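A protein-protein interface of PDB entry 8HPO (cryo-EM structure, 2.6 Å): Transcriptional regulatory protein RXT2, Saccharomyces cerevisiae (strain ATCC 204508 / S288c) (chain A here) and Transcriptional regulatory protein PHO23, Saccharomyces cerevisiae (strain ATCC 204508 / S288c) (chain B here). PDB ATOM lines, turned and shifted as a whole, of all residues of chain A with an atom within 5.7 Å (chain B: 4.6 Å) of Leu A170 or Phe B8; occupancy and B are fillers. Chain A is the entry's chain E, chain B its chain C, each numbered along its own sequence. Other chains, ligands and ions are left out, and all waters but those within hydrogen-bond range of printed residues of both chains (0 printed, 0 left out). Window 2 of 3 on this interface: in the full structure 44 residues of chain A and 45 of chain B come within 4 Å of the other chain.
The backbone NH (N) of Ile A169 is in hydrogen-bond range of the side-chain amide oxygen (OD1) of Asn B12, at 3.3 Å.
Leu A170 touches just one residue of chain B: Phe B8 (3.9 Å). Phe B8 touches just these residues of chain A: Ile A169, Leu A170 and SEP A171. Of the printed residues of chain B, Ile A169 touches Phe B8, Leu B11 and Asn B12. Printed residues of chain A within 4 Å of Glu B116: Leu A172 (3.8 Å). Of the printed residues of chain A, Leu B11 touches Ile A169. The nearest residue of chain A that does not touch Phe B8 is Leu A172 (4.1 Å). The nearest printed residue of chain B that does not touch Leu A172 is Phe B8 (4.1 Å).
N of SEP A171 lies within hydrogen-bond range of the side-chain carboxylate of Asp A174 (2.8 Å). N of Phe B8 sits close to OD1 of Asn B6 (3.4 Å). The backbone NH (N) of Leu B11 sits at hydrogen-bond distance from the side-chain carboxylate (OE1) of Glu B116. The backbone NH (N) of Gly B10 is in hydrogen-bond range of the side-chain carboxylate (OE1) of Glu B116 (2.9 Å).
Hydrophobic or aromatic side chains of chain B that line the printed part of chain A: Phe B8. Of the 7 printed residues of chain A, 5 touch a printed residue of chain B. Printed residues of chain A that touch a printed residue of chain B: Pro A168, Ile A169, Leu A170, SEP A171 and Leu A172. Among the printed residues, 7 pairs touch across the chains. Among the printed residues, no Asp or Glu carboxylate lies within 4 Å of a Lys or Arg side-chain nitrogen of the other chain.
Asn B12 touches Pro A168 (OD1 to CA, 3.4 Å). Phe B8 touches Ile A169 (CD1 to CG2, 3.9 Å). CD1 of Ile A169 touches O of Leu B11, at 3.95 Å. CE2 of Phe B8 touches O of Leu A170, 3.9 Å away. O2P of SEP A171 touches CZ of Phe B8 (3.5 Å). Glu B116 touches Leu A172.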
ATOM      1  N   TPO A 167      -5.875 -14.931  28.855  1.00  0.00           N
ATOM      2  CA  TPO A 167      -7.344 -14.743  28.751  1.00  0.00           C
ATOM      3  CB  TPO A 167      -7.842 -14.099  27.491  1.00  0.00           C
ATOM      4  CG2 TPO A 167      -8.784 -12.954  27.746  1.00  0.00           C
ATOM      5  OG1 TPO A 167      -6.729 -13.586  26.854  1.00  0.00           O
ATOM      6  P   TPO A 167      -7.073 -12.704  25.770  1.00  0.00           P
ATOM      7  O1P TPO A 167      -8.369 -13.191  25.118  1.00  0.00           O
ATOM      8  O2P TPO A 167      -5.819 -12.914  24.997  1.00  0.00           O
ATOM      9  O3P TPO A 167      -7.150 -11.354  26.378  1.00  0.00           O
ATOM     10  C   TPO A 167      -8.129 -15.991  28.356  1.00  0.00           C
ATOM     11  O   TPO A 167      -7.653 -16.838  27.619  1.00  0.00           O
ATOM     12  N   PRO A 168      -9.425 -15.954  28.617  1.00  0.00           N
ATOM     13  CA  PRO A 168     -10.278 -17.039  28.369  1.00  0.00           C
ATOM     14  C   PRO A 168     -10.498 -17.489  26.926  1.00  0.00           C
ATOM     15  O   PRO A 168     -10.232 -16.810  26.059  1.00  0.00           O
ATOM     16  CB  PRO A 168     -11.557 -16.373  28.926  1.00  0.00           C
ATOM     17  CG  PRO A 168     -11.403 -14.957  28.648  1.00  0.00           C
ATOM     18  CD  PRO A 168     -10.050 -14.818  29.227  1.00  0.00           C
ATOM     19  N   ILE A 169     -11.010 -18.692  26.774  1.00  0.00           N
ATOM     20  CA  ILE A 169     -11.479 -19.329  25.537  1.00  0.00           C
ATOM     21  C   ILE A 169     -12.613 -18.444  25.031  1.00  0.00           C
ATOM     22  O   ILE A 169     -13.413 -18.003  25.779  1.00  0.00           O
ATOM     23  CB  ILE A 169     -11.866 -20.779  25.865  1.00  0.00           C
ATOM     24  CG1 ILE A 169     -10.708 -21.747  25.773  1.00  0.00           C
ATOM     25  CG2 ILE A 169     -12.981 -21.295  25.047  1.00  0.00           C
ATOM     26  CD1 ILE A 169     -10.654 -22.733  26.891  1.00  0.00           C
ATOM     27  N   LEU A 170     -12.680 -18.235  23.735  1.00  0.00           N
ATOM     28  CA  LEU A 170     -13.707 -17.374  23.174  1.00  0.00           C
ATOM     29  C   LEU A 170     -14.543 -18.234  22.278  1.00  0.00           C
ATOM     30  O   LEU A 170     -15.613 -17.792  21.930  1.00  0.00           O
ATOM     31  CB  LEU A 170     -13.006 -16.321  22.323  1.00  0.00           C
ATOM     32  CG  LEU A 170     -12.340 -15.192  23.088  1.00  0.00           C
ATOM     33  CD1 LEU A 170     -11.093 -14.726  22.378  1.00  0.00           C
ATOM     34  CD2 LEU A 170     -13.317 -14.061  23.304  1.00  0.00           C
ATOM     35  N   SEP A 171     -14.028 -19.402  21.939  1.00  0.00           N
ATOM     36  CA  SEP A 171     -14.780 -20.319  21.050  1.00  0.00           C
ATOM     37  CB  SEP A 171     -14.744 -19.846  19.646  1.00  0.00           C
ATOM     38  OG  SEP A 171     -16.110 -19.659  19.235  1.00  0.00           O
ATOM     39  C   SEP A 171     -14.202 -21.725  21.137  1.00  0.00           C
ATOM     40  O   SEP A 171     -13.320 -21.939  21.911  1.00  0.00           O
ATOM     41  P   SEP A 171     -17.055 -20.878  18.767  1.00  0.00           P
ATOM     42  O1P SEP A 171     -16.572 -21.384  17.427  1.00  0.00           O
ATOM     43  O2P SEP A 171     -17.141 -21.963  19.816  1.00  0.00           O
ATOM     44  O3P SEP A 171     -18.352 -20.141  18.624  1.00  0.00           O
ATOM     45  N   LEU A 172     -14.795 -22.683  20.454  1.00  0.00           N
ATOM     46  CA  LEU A 172     -14.225 -24.035  20.483  1.00  0.00           C
ATOM     47  C   LEU A 172     -12.874 -24.054  19.767  1.00  0.00           C
ATOM     48  O   LEU A 172     -11.973 -24.599  20.302  1.00  0.00           O
ATOM     49  CB  LEU A 172     -15.253 -24.941  19.837  1.00  0.00           C
ATOM     50  CG  LEU A 172     -15.071 -26.416  20.113  1.00  0.00           C
ATOM     51  CD1 LEU A 172     -14.411 -26.654  21.444  1.00  0.00           C
ATOM     52  CD2 LEU A 172     -16.403 -27.110  20.015  1.00  0.00           C
ATOM     53  N   ASP A 174     -10.471 -22.404  19.906  1.00  0.00           N
ATOM     54  CA  ASP A 174      -9.329 -21.884  20.645  1.00  0.00           C
ATOM     55  C   ASP A 174      -8.536 -22.965  21.358  1.00  0.00           C
ATOM     56  O   ASP A 174      -7.507 -22.656  21.962  1.00  0.00           O
ATOM     57  CB  ASP A 174      -9.788 -20.838  21.657  1.00  0.00           C
ATOM     58  CG  ASP A 174     -10.495 -19.679  21.004  1.00  0.00           C
ATOM     59  OD1 ASP A 174      -9.911 -18.580  20.943  1.00  0.00           O
ATOM     60  OD2 ASP A 174     -11.637 -19.873  20.542  1.00  0.00           O
ATOM     61  N   ASN B   6     -22.204 -16.139  25.867  1.00  0.00           N
ATOM     62  CA  ASN B   6     -21.645 -17.422  26.277  1.00  0.00           C
ATOM     63  C   ASN B   6     -20.176 -17.188  26.607  1.00  0.00           C
ATOM     64  O   ASN B   6     -19.341 -17.114  25.705  1.00  0.00           O
ATOM     65  CB  ASN B   6     -21.816 -18.468  25.187  1.00  0.00           C
ATOM     66  CG  ASN B   6     -21.795 -19.879  25.724  1.00  0.00           C
ATOM     67  OD1 ASN B   6     -20.748 -20.393  26.111  1.00  0.00           O
ATOM     68  ND2 ASN B   6     -22.955 -20.517  25.747  1.00  0.00           N
ATOM     69  N   LEU B   7     -19.873 -17.066  27.896  1.00  0.00           N
ATOM     70  CA  LEU B   7     -18.513 -16.818  28.344  1.00  0.00           C
ATOM     71  C   LEU B   7     -17.697 -18.093  28.485  1.00  0.00           C
ATOM     72  O   LEU B   7     -16.567 -18.029  28.976  1.00  0.00           O
ATOM     73  CB  LEU B   7     -18.525 -16.059  29.673  1.00  0.00           C
ATOM     74  CG  LEU B   7     -18.678 -14.534  29.650  1.00  0.00           C
ATOM     75  CD1 LEU B   7     -17.642 -13.902  28.750  1.00  0.00           C
ATOM     76  CD2 LEU B   7     -20.074 -14.111  29.233  1.00  0.00           C
ATOM     77  N   PHE B   8     -18.245 -19.232  28.071  1.00  0.00           N
ATOM     78  CA  PHE B   8     -17.531 -20.503  28.035  1.00  0.00           C
ATOM     79  C   PHE B   8     -16.906 -20.883  29.382  1.00  0.00           C
ATOM     80  O   PHE B   8     -15.694 -21.096  29.469  1.00  0.00           O
ATOM     81  CB  PHE B   8     -16.477 -20.483  26.937  1.00  0.00           C
ATOM     82  CG  PHE B   8     -17.042 -20.696  25.563  1.00  0.00           C
ATOM     83  CD1 PHE B   8     -16.801 -21.861  24.872  1.00  0.00           C
ATOM     84  CD2 PHE B   8     -17.844 -19.736  24.978  1.00  0.00           C
ATOM     85  CE1 PHE B   8     -17.343 -22.061  23.629  1.00  0.00           C
ATOM     86  CE2 PHE B   8     -18.387 -19.931  23.734  1.00  0.00           C
ATOM     87  CZ  PHE B   8     -18.136 -21.092  23.060  1.00  0.00           C
ATOM     88  N   PRO B   9     -17.713 -20.998  30.446  1.00  0.00           N
ATOM     89  CA  PRO B   9     -17.124 -21.292  31.763  1.00  0.00           C
ATOM     90  C   PRO B   9     -16.726 -22.745  31.932  1.00  0.00           C
ATOM     91  O   PRO B   9     -15.740 -23.041  32.624  1.00  0.00           O
ATOM     92  CB  PRO B   9     -18.238 -20.889  32.734  1.00  0.00           C
ATOM     93  CG  PRO B   9     -19.483 -21.039  31.968  1.00  0.00           C
ATOM     94  CD  PRO B   9     -19.175 -20.845  30.517  1.00  0.00           C
ATOM     95  N   GLY B  10     -17.474 -23.664  31.318  1.00  0.00           N
ATOM     96  CA  GLY B  10     -17.110 -25.068  31.373  1.00  0.00           C
ATOM     97  C   GLY B  10     -15.700 -25.325  30.887  1.00  0.00           C
ATOM     98  O   GLY B  10     -14.888 -25.918  31.596  1.00  0.00           O
ATOM     99  N   LEU B  11     -15.386 -24.870  29.673  1.00  0.00           N
ATOM    100  CA  LEU B  11     -14.075 -25.144  29.091  1.00  0.00           C
ATOM    101  C   LEU B  11     -12.958 -24.439  29.849  1.00  0.00           C
ATOM    102  O   LEU B  11     -11.838 -24.958  29.934  1.00  0.00           O
ATOM    103  CB  LEU B  11     -14.061 -24.741  27.621  1.00  0.00           C
ATOM    104  CG  LEU B  11     -15.137 -25.351  26.726  1.00  0.00           C
ATOM    105  CD1 LEU B  11     -14.965 -24.848  25.316  1.00  0.00           C
ATOM    106  CD2 LEU B  11     -15.064 -26.860  26.757  1.00  0.00           C
ATOM    107  N   ASN B  12     -13.244 -23.282  30.442  1.00  0.00           N
ATOM    108  CA  ASN B  12     -12.212 -22.578  31.198  1.00  0.00           C
ATOM    109  C   ASN B  12     -11.879 -23.312  32.493  1.00  0.00           C
ATOM    110  O   ASN B  12     -10.696 -23.517  32.824  1.00  0.00           O
ATOM    111  CB  ASN B  12     -12.669 -21.150  31.476  1.00  0.00           C
ATOM    112  CG  ASN B  12     -12.591 -20.260  30.244  1.00  0.00           C
ATOM    113  OD1 ASN B  12     -11.523 -19.774  29.888  1.00  0.00           O
ATOM    114  ND2 ASN B  12     -13.726 -20.038  29.600  1.00  0.00           N
ATOM    115  N   GLU B 116     -21.064 -24.848  24.771  1.00  0.00           N
ATOM    116  CA  GLU B 116     -19.644 -24.752  24.482  1.00  0.00           C
ATOM    117  C   GLU B 116     -19.158 -25.910  23.629  1.00  0.00           C
ATOM    118  O   GLU B 116     -17.988 -25.927  23.237  1.00  0.00           O
ATOM    119  CB  GLU B 116     -18.857 -24.681  25.788  1.00  0.00           C
ATOM    120  CG  GLU B 116     -19.338 -23.566  26.687  1.00  0.00           C
ATOM    121  CD  GLU B 116     -19.214 -23.893  28.146  1.00  0.00           C
ATOM    122  OE1 GLU B 116     -18.123 -24.318  28.565  1.00  0.00           O
ATOM    123  OE2 GLU B 116     -20.208 -23.717  28.876  1.00  0.00           O
